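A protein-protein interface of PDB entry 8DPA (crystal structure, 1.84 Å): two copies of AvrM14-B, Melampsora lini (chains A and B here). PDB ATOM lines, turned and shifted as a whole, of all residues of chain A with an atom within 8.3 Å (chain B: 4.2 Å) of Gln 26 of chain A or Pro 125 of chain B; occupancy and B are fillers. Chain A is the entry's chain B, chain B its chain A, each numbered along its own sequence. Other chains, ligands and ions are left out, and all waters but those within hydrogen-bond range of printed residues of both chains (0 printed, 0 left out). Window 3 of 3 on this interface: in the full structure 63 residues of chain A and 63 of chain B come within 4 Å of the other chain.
No position is printed for both chains. Of the 11 pairs that touch across the chains among the printed residues, none has its exchanged pair printed and touching as well.
Among the printed residues, pairs that only touch across the chains: Gln 26 of chain A with Pro 125 of chain B (3.3 Å), Gln 26 of chain A with Phe 148 of chain B (3.4 Å), Tyr 18 of chain A with Phe 148 of chain B (3.6 Å), Ile 100 of chain A with Phe 148 of chain B (3.7 Å), Phe 44 of chain A with Trp 141 of chain B (3.7 Å), Val 28 of chain A with Phe 148 of chain B (3.8 Å), Phe 44 of chain A with Val 128 of chain B (3.8 Å), Val 28 of chain A with Val 128 of chain B (3.9 Å) and Leu 30 of chain A with Val 123 of chain B (3.9 Å).
O of Val 123 of chain B sits at hydrogen-bond distance from N of Val 28 of chain A (2.7 Å). The backbone carbonyl oxygen of Val 123 of chain B lies within hydrogen-bond range of the side-chain hydroxyl of Thr 27 of chain A (2.8 Å).
Of the printed residues of chain B, Val 28 of chain A touches Val 123, Val 128 and Phe 148. Printed residues of chain B within 4 Å of Phe 44 of chain A: Val 128 and Trp 141. Pro 125 of chain B touches one residue of chain A. Ser 126 of chain B touches none of the printed residues of chain A. Printed residues of chain A within 4 Å of Val 128 of chain B: Val 28 (3.9 Å) and Phe 44 (3.8 Å). The nearest printed residue of chain B that does not touch Gln 26 of chain A is Arg 124 of chain B (4.3 Å). The nearest residue of chain A that does not touch Pro 125 of chain B is Val 28 of chain A (4.1 Å).
OE2 of Glu 20 of chain A sits at hydrogen-bond distance from NE2 of Gln 26 of chain A. N of Arg 19 of chain A lies within hydrogen-bond range of O of Thr 27 of chain A, at 2.9 Å.
Of the 8 printed residues of chain B, 5 touch a printed residue of chain A. Of the 18 printed residues of chain A, 7 touch a printed residue of chain B. Hydrophobic or aromatic side chains of chain A within 4 Å of the printed part of chain B: Tyr 18, Val 28, Leu 30, Phe 44 and Ile 100. Among the printed residues, 11 pairs touch across the chains.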
ATOM      1  N   VAL A  17       6.379  33.867 -10.577  1.00  0.00           N
ATOM      2  CA  VAL A  17       6.189  33.859 -12.023  1.00  0.00           C
ATOM      3  C   VAL A  17       5.590  32.519 -12.425  1.00  0.00           C
ATOM      4  O   VAL A  17       6.055  31.464 -11.974  1.00  0.00           O
ATOM      5  CB  VAL A  17       7.520  34.110 -12.753  1.00  0.00           C
ATOM      6  CG1 VAL A  17       7.333  33.963 -14.261  1.00  0.00           C
ATOM      7  CG2 VAL A  17       8.070  35.498 -12.397  1.00  0.00           C
ATOM      8  N   TYR A  18       4.551  32.552 -13.253  1.00  0.00           N
ATOM      9  CA  TYR A  18       3.932  31.314 -13.705  1.00  0.00           C
ATOM     10  C   TYR A  18       3.518  31.453 -15.158  1.00  0.00           C
ATOM     11  O   TYR A  18       3.419  32.555 -15.698  1.00  0.00           O
ATOM     12  CB  TYR A  18       2.707  30.928 -12.857  1.00  0.00           C
ATOM     13  CG  TYR A  18       1.437  31.628 -13.268  1.00  0.00           C
ATOM     14  CD1 TYR A  18       1.183  32.937 -12.864  1.00  0.00           C
ATOM     15  CD2 TYR A  18       0.495  30.989 -14.062  1.00  0.00           C
ATOM     16  CE1 TYR A  18       0.027  33.585 -13.238  1.00  0.00           C
ATOM     17  CE2 TYR A  18      -0.664  31.635 -14.448  1.00  0.00           C
ATOM     18  CZ  TYR A  18      -0.893  32.933 -14.033  1.00  0.00           C
ATOM     19  OH  TYR A  18      -2.043  33.578 -14.417  1.00  0.00           O
ATOM     20  N   ARG A  19       3.259  30.318 -15.795  1.00  0.00           N
ATOM     21  CA  ARG A  19       2.619  30.354 -17.100  1.00  0.00           C
ATOM     22  C   ARG A  19       1.576  29.260 -17.179  1.00  0.00           C
ATOM     23  O   ARG A  19       1.623  28.277 -16.433  1.00  0.00           O
ATOM     24  CB  ARG A  19       3.650  30.270 -18.223  1.00  0.00           C
ATOM     25  CG  ARG A  19       4.457  29.047 -18.258  1.00  0.00           C
ATOM     26  CD  ARG A  19       5.464  29.215 -19.395  1.00  0.00           C
ATOM     27  NE  ARG A  19       6.419  28.126 -19.423  1.00  0.00           N
ATOM     28  CZ  ARG A  19       7.540  28.130 -20.135  1.00  0.00           C
ATOM     29  NH1 ARG A  19       7.882  29.165 -20.890  1.00  0.00           N
ATOM     30  NH2 ARG A  19       8.355  27.088 -20.052  1.00  0.00           N
ATOM     31  N   GLU A  20       0.583  29.500 -18.029  1.00  0.00           N
ATOM     32  CA  GLU A  20      -0.448  28.516 -18.303  1.00  0.00           C
ATOM     33  C   GLU A  20      -0.026  27.687 -19.496  1.00  0.00           C
ATOM     34  O   GLU A  20       0.399  28.236 -20.516  1.00  0.00           O
ATOM     35  CB  GLU A  20      -1.799  29.170 -18.573  1.00  0.00           C
ATOM     36  CG  GLU A  20      -2.261  30.004 -17.423  1.00  0.00           C
ATOM     37  CD  GLU A  20      -3.524  29.429 -16.812  1.00  0.00           C
ATOM     38  OE1 GLU A  20      -3.921  28.312 -17.214  1.00  0.00           O
ATOM     39  OE2 GLU A  20      -4.082  30.074 -15.899  1.00  0.00           O
ATOM     40  N   LEU A  21      -0.133  26.373 -19.354  1.00  0.00           N
ATOM     41  CA  LEU A  21       0.220  25.446 -20.411  1.00  0.00           C
ATOM     42  C   LEU A  21      -1.021  25.105 -21.224  1.00  0.00           C
ATOM     43  O   LEU A  21      -2.152  25.354 -20.798  1.00  0.00           O
ATOM     44  CB  LEU A  21       0.842  24.183 -19.820  1.00  0.00           C
ATOM     45  CG  LEU A  21       2.136  24.441 -19.041  1.00  0.00           C
ATOM     46  CD1 LEU A  21       2.625  23.158 -18.387  1.00  0.00           C
ATOM     47  CD2 LEU A  21       3.209  25.059 -19.925  1.00  0.00           C
ATOM     48  N   SER A  22      -0.791  24.523 -22.406  1.00  0.00           N
ATOM     49  CA  SER A  22      -1.881  24.282 -23.349  1.00  0.00           C
ATOM     50  C   SER A  22      -2.946  23.353 -22.777  1.00  0.00           C
ATOM     51  O   SER A  22      -4.128  23.494 -23.111  1.00  0.00           O
ATOM     52  CB  SER A  22      -1.328  23.708 -24.655  1.00  0.00           C
ATOM     53  OG  SER A  22      -0.525  22.570 -24.408  1.00  0.00           O
ATOM     54  N   ASP A  23      -2.561  22.397 -21.929  1.00  0.00           N
ATOM     55  CA  ASP A  23      -3.545  21.527 -21.297  1.00  0.00           C
ATOM     56  C   ASP A  23      -4.252  22.191 -20.116  1.00  0.00           C
ATOM     57  O   ASP A  23      -4.884  21.491 -19.318  1.00  0.00           O
ATOM     58  CB  ASP A  23      -2.898  20.210 -20.852  1.00  0.00           C
ATOM     59  CG  ASP A  23      -1.618  20.415 -20.063  1.00  0.00           C
ATOM     60  OD1 ASP A  23      -1.490  21.451 -19.380  1.00  0.00           O
ATOM     61  OD2 ASP A  23      -0.740  19.529 -20.117  1.00  0.00           O
ATOM     62  N   GLY A  24      -4.162  23.516 -19.987  1.00  0.00           N
ATOM     63  CA  GLY A  24      -4.835  24.247 -18.931  1.00  0.00           C
ATOM     64  C   GLY A  24      -4.128  24.274 -17.592  1.00  0.00           C
ATOM     65  O   GLY A  24      -4.577  24.995 -16.688  1.00  0.00           O
ATOM     66  N   SER A  25      -3.046  23.519 -17.425  1.00  0.00           N
ATOM     67  CA  SER A  25      -2.348  23.497 -16.151  1.00  0.00           C
ATOM     68  C   SER A  25      -1.348  24.647 -16.070  1.00  0.00           C
ATOM     69  O   SER A  25      -1.046  25.328 -17.053  1.00  0.00           O
ATOM     70  CB  SER A  25      -1.623  22.170 -15.954  1.00  0.00           C
ATOM     71  OG  SER A  25      -0.714  21.954 -17.014  1.00  0.00           O
ATOM     72  N   GLN A  26      -0.817  24.851 -14.875  1.00  0.00           N
ATOM     73  CA  GLN A  26       0.103  25.943 -14.624  1.00  0.00           C
ATOM     74  C   GLN A  26       1.439  25.406 -14.141  1.00  0.00           C
ATOM     75  O   GLN A  26       1.529  24.314 -13.578  1.00  0.00           O
ATOM     76  CB  GLN A  26      -0.487  26.922 -13.606  1.00  0.00           C
ATOM     77  CG  GLN A  26      -1.972  27.071 -13.799  1.00  0.00           C
ATOM     78  CD  GLN A  26      -2.665  27.711 -12.637  1.00  0.00           C
ATOM     79  OE1 GLN A  26      -2.667  27.171 -11.527  1.00  0.00           O
ATOM     80  NE2 GLN A  26      -3.296  28.857 -12.883  1.00  0.00           N
ATOM     81  N   THR A  27       2.475  26.181 -14.393  1.00  0.00           N
ATOM     82  CA  THR A  27       3.809  25.902 -13.899  1.00  0.00           C
ATOM     83  C   THR A  27       4.431  27.187 -13.370  1.00  0.00           C
ATOM     84  O   THR A  27       4.160  28.273 -13.883  1.00  0.00           O
ATOM     85  CB  THR A  27       4.657  25.262 -14.999  1.00  0.00           C
ATOM     86  OG1 THR A  27       5.837  24.687 -14.424  1.00  0.00           O
ATOM     87  CG2 THR A  27       4.979  26.247 -16.094  1.00  0.00           C
ATOM     88  N   VAL A  28       5.257  27.043 -12.329  1.00  0.00           N
ATOM     89  CA  VAL A  28       5.820  28.153 -11.558  1.00  0.00           C
ATOM     90  C   VAL A  28       7.331  28.155 -11.730  1.00  0.00           C
ATOM     91  O   VAL A  28       7.973  27.100 -11.629  1.00  0.00           O
ATOM     92  CB  VAL A  28       5.453  28.038 -10.065  1.00  0.00           C
ATOM     93  CG1 VAL A  28       6.163  29.126  -9.228  1.00  0.00           C
ATOM     94  CG2 VAL A  28       3.929  28.079  -9.883  1.00  0.00           C
ATOM     95  N   LEU A  29       7.899  29.332 -11.975  1.00  0.00           N
ATOM     96  CA  LEU A  29       9.334  29.476 -12.196  1.00  0.00           C
ATOM     97  C   LEU A  29      10.089  29.658 -10.882  1.00  0.00           C
ATOM     98  O   LEU A  29       9.777  30.557 -10.102  1.00  0.00           O
ATOM     99  CB  LEU A  29       9.602  30.670 -13.111  1.00  0.00           C
ATOM    100  CG  LEU A  29      11.064  30.844 -13.495  1.00  0.00           C
ATOM    101  CD1 LEU A  29      11.522  29.666 -14.341  1.00  0.00           C
ATOM    102  CD2 LEU A  29      11.240  32.129 -14.264  1.00  0.00           C
ATOM    103  N   LEU A  30      11.092  28.822 -10.646  1.00  0.00           N
ATOM    104  CA  LEU A  30      11.954  28.959  -9.479  1.00  0.00           C
ATOM    105  C   LEU A  30      13.365  29.271  -9.948  1.00  0.00           C
ATOM    106  O   LEU A  30      13.751  28.928 -11.073  1.00  0.00           O
ATOM    107  CB  LEU A  30      11.966  27.687  -8.634  1.00  0.00           C
ATOM    108  CG  LEU A  30      10.642  27.332  -7.960  1.00  0.00           C
ATOM    109  CD1 LEU A  30      10.778  26.019  -7.210  1.00  0.00           C
ATOM    110  CD2 LEU A  30      10.170  28.463  -7.008  1.00  0.00           C
ATOM    111  N   PHE A  44      11.939  32.747  -5.570  1.00  0.00           N
ATOM    112  CA  PHE A  44      11.212  33.453  -6.613  1.00  0.00           C
ATOM    113  C   PHE A  44      12.081  34.584  -7.154  1.00  0.00           C
ATOM    114  O   PHE A  44      13.218  34.778  -6.727  1.00  0.00           O
ATOM    115  CB  PHE A  44       9.885  33.973  -6.071  1.00  0.00           C
ATOM    116  CG  PHE A  44       9.011  32.896  -5.480  1.00  0.00           C
ATOM    117  CD1 PHE A  44       8.546  31.843  -6.270  1.00  0.00           C
ATOM    118  CD2 PHE A  44       8.642  32.940  -4.141  1.00  0.00           C
ATOM    119  CE1 PHE A  44       7.735  30.850  -5.727  1.00  0.00           C
ATOM    120  CE2 PHE A  44       7.829  31.957  -3.591  1.00  0.00           C
ATOM    121  CZ  PHE A  44       7.372  30.908  -4.378  1.00  0.00           C
ATOM    122  N   ILE A 100       1.872  37.900  -7.970  1.00  0.00           N
ATOM    123  CA  ILE A 100       1.785  36.834  -8.962  1.00  0.00           C
ATOM    124  C   ILE A 100       1.946  37.482 -10.327  1.00  0.00           C
ATOM    125  O   ILE A 100       1.262  38.464 -10.630  1.00  0.00           O
ATOM    126  CB  ILE A 100       0.439  36.097  -8.877  1.00  0.00           C
ATOM    127  CG1 ILE A 100       0.222  35.474  -7.484  1.00  0.00           C
ATOM    128  CG2 ILE A 100       0.326  35.055 -10.030  1.00  0.00           C
ATOM    129  CD1 ILE A 100       0.724  34.106  -7.327  1.00  0.00           C
ATOM    130  N   GLN A 102       2.091  36.606 -14.471  1.00  0.00           N
ATOM    131  CA  GLN A 102       1.894  35.653 -15.562  1.00  0.00           C
ATOM    132  C   GLN A 102       2.773  36.021 -16.747  1.00  0.00           C
ATOM    133  O   GLN A 102       2.757  37.167 -17.209  1.00  0.00           O
ATOM    134  CB  GLN A 102       0.428  35.611 -16.001  1.00  0.00           C
ATOM    135  CG  GLN A 102       0.154  34.514 -17.054  1.00  0.00           C
ATOM    136  CD  GLN A 102      -1.256  34.564 -17.588  1.00  0.00           C
ATOM    137  OE1 GLN A 102      -1.938  35.575 -17.444  1.00  0.00           O
ATOM    138  NE2 GLN A 102      -1.679  33.497 -18.277  1.00  0.00           N
ATOM    139  N   VAL A 116       9.837  23.015 -19.004  1.00  0.00           N
ATOM    140  CA  VAL A 116       9.419  22.229 -17.847  1.00  0.00           C
ATOM    141  C   VAL A 116      10.459  21.162 -17.507  1.00  0.00           C
ATOM    142  O   VAL A 116      10.795  20.950 -16.340  1.00  0.00           O
ATOM    143  CB  VAL A 116       8.032  21.586 -18.081  1.00  0.00           C
ATOM    144  CG1 VAL A 116       7.887  20.286 -17.290  1.00  0.00           C
ATOM    145  CG2 VAL A 116       6.927  22.559 -17.706  1.00  0.00           C
ATOM    146  N   VAL B 123       8.332  24.329 -12.228  1.00  0.00           N
ATOM    147  CA  VAL B 123       7.749  23.230 -11.461  1.00  0.00           C
ATOM    148  C   VAL B 123       6.232  23.379 -11.365  1.00  0.00           C
ATOM    149  O   VAL B 123       5.666  24.450 -11.599  1.00  0.00           O
ATOM    150  CB  VAL B 123       8.358  23.126 -10.045  1.00  0.00           C
ATOM    151  CG1 VAL B 123       9.886  23.041 -10.110  1.00  0.00           C
ATOM    152  CG2 VAL B 123       7.917  24.302  -9.186  1.00  0.00           C
ATOM    153  N   ARG B 124       5.576  22.333 -10.932  1.00  0.00           N
ATOM    154  CA  ARG B 124       4.153  22.440 -10.731  1.00  0.00           C
ATOM    155  C   ARG B 124       3.939  23.132  -9.377  1.00  0.00           C
ATOM    156  O   ARG B 124       4.784  23.048  -8.522  1.00  0.00           O
ATOM    157  CB  ARG B 124       3.507  21.064 -10.687  1.00  0.00           C
ATOM    158  CG  ARG B 124       3.515  20.329 -12.019  1.00  0.00           C
ATOM    159  CD  ARG B 124       2.891  18.957 -11.894  1.00  0.00           C
ATOM    160  NE  ARG B 124       3.501  18.194 -10.819  1.00  0.00           N
ATOM    161  CZ  ARG B 124       4.526  17.366 -10.965  1.00  0.00           C
ATOM    162  NH1 ARG B 124       5.072  17.163 -12.163  1.00  0.00           N
ATOM    163  NH2 ARG B 124       5.011  16.728  -9.913  1.00  0.00           N
ATOM    164  N   PRO B 125       2.817  23.826  -9.221  1.00  0.00           N
ATOM    165  CA  PRO B 125       2.507  24.432  -7.911  1.00  0.00           C
ATOM    166  C   PRO B 125       2.669  23.485  -6.730  1.00  0.00           C
ATOM    167  O   PRO B 125       3.140  23.914  -5.669  1.00  0.00           O
ATOM    168  CB  PRO B 125       1.049  24.879  -8.094  1.00  0.00           C
ATOM    169  CG  PRO B 125       1.005  25.284  -9.543  1.00  0.00           C
ATOM    170  CD  PRO B 125       1.867  24.272 -10.263  1.00  0.00           C
ATOM    171  N   SER B 126       2.326  22.202  -6.885  1.00  0.00           N
ATOM    172  CA  SER B 126       2.392  21.270  -5.765  1.00  0.00           C
ATOM    173  C   SER B 126       3.825  20.964  -5.354  1.00  0.00           C
ATOM    174  O   SER B 126       4.030  20.386  -4.283  1.00  0.00           O
ATOM    175  CB  SER B 126       1.719  19.937  -6.095  1.00  0.00           C
ATOM    176  OG  SER B 126       2.241  19.406  -7.313  1.00  0.00           O
ATOM    177  N   GLU B 127       4.813  21.297  -6.189  1.00  0.00           N
ATOM    178  CA  GLU B 127       6.214  21.044  -5.875  1.00  0.00           C
ATOM    179  C   GLU B 127       6.948  22.268  -5.339  1.00  0.00           C
ATOM    180  O   GLU B 127       8.121  22.143  -4.966  1.00  0.00           O
ATOM    181  CB  GLU B 127       6.973  20.532  -7.109  1.00  0.00           C
ATOM    182  CG  GLU B 127       6.188  19.668  -8.072  1.00  0.00           C
ATOM    183  CD  GLU B 127       7.015  19.307  -9.307  1.00  0.00           C
ATOM    184  OE1 GLU B 127       8.042  18.616  -9.145  1.00  0.00           O
ATOM    185  OE2 GLU B 127       6.666  19.744 -10.427  1.00  0.00           O
ATOM    186  N   VAL B 128       6.298  23.437  -5.303  1.00  0.00           N
ATOM    187  CA  VAL B 128       7.000  24.677  -4.975  1.00  0.00           C
ATOM    188  C   VAL B 128       7.486  24.660  -3.533  1.00  0.00           C
ATOM    189  O   VAL B 128       8.654  24.958  -3.250  1.00  0.00           O
ATOM    190  CB  VAL B 128       6.100  25.901  -5.232  1.00  0.00           C
ATOM    191  CG1 VAL B 128       6.716  27.146  -4.615  1.00  0.00           C
ATOM    192  CG2 VAL B 128       5.893  26.118  -6.735  1.00  0.00           C
ATOM    193  N   TRP B 141       4.984  32.762  -0.624  1.00  0.00           N
ATOM    194  CA  TRP B 141       4.178  31.634  -1.076  1.00  0.00           C
ATOM    195  C   TRP B 141       2.964  31.430  -0.174  1.00  0.00           C
ATOM    196  O   TRP B 141       1.864  31.133  -0.654  1.00  0.00           O
ATOM    197  CB  TRP B 141       5.042  30.371  -1.118  1.00  0.00           C
ATOM    198  CG  TRP B 141       4.338  29.145  -1.655  1.00  0.00           C
ATOM    199  CD1 TRP B 141       4.049  27.991  -0.972  1.00  0.00           C
ATOM    200  CD2 TRP B 141       3.854  28.951  -2.990  1.00  0.00           C
ATOM    201  NE1 TRP B 141       3.411  27.098  -1.800  1.00  0.00           N
ATOM    202  CE2 TRP B 141       3.269  27.663  -3.042  1.00  0.00           C
ATOM    203  CE3 TRP B 141       3.842  29.746  -4.140  1.00  0.00           C
ATOM    204  CZ2 TRP B 141       2.703  27.136  -4.213  1.00  0.00           C
ATOM    205  CZ3 TRP B 141       3.267  29.223  -5.308  1.00  0.00           C
ATOM    206  CH2 TRP B 141       2.705  27.929  -5.328  1.00  0.00           C
ATOM    207  N   PHE B 148      -3.254  29.528  -7.130  1.00  0.00           N
ATOM    208  CA  PHE B 148      -3.048  28.333  -7.990  1.00  0.00           C
ATOM    209  C   PHE B 148      -4.031  27.208  -7.634  1.00  0.00           C
ATOM    210  O   PHE B 148      -4.874  27.457  -6.709  1.00  0.00           O
ATOM    211  CB  PHE B 148      -1.628  27.834  -7.862  1.00  0.00           C
ATOM    212  CG  PHE B 148      -0.617  28.825  -8.333  1.00  0.00           C
ATOM    213  CD1 PHE B 148      -0.458  29.049  -9.701  1.00  0.00           C
ATOM    214  CD2 PHE B 148       0.150  29.545  -7.433  1.00  0.00           C
ATOM    215  CE1 PHE B 148       0.462  29.964 -10.162  1.00  0.00           C
ATOM    216  CE2 PHE B 148       1.075  30.477  -7.888  1.00  0.00           C
ATOM    217  CZ  PHE B 148       1.229  30.693  -9.259  1.00  0.00           C
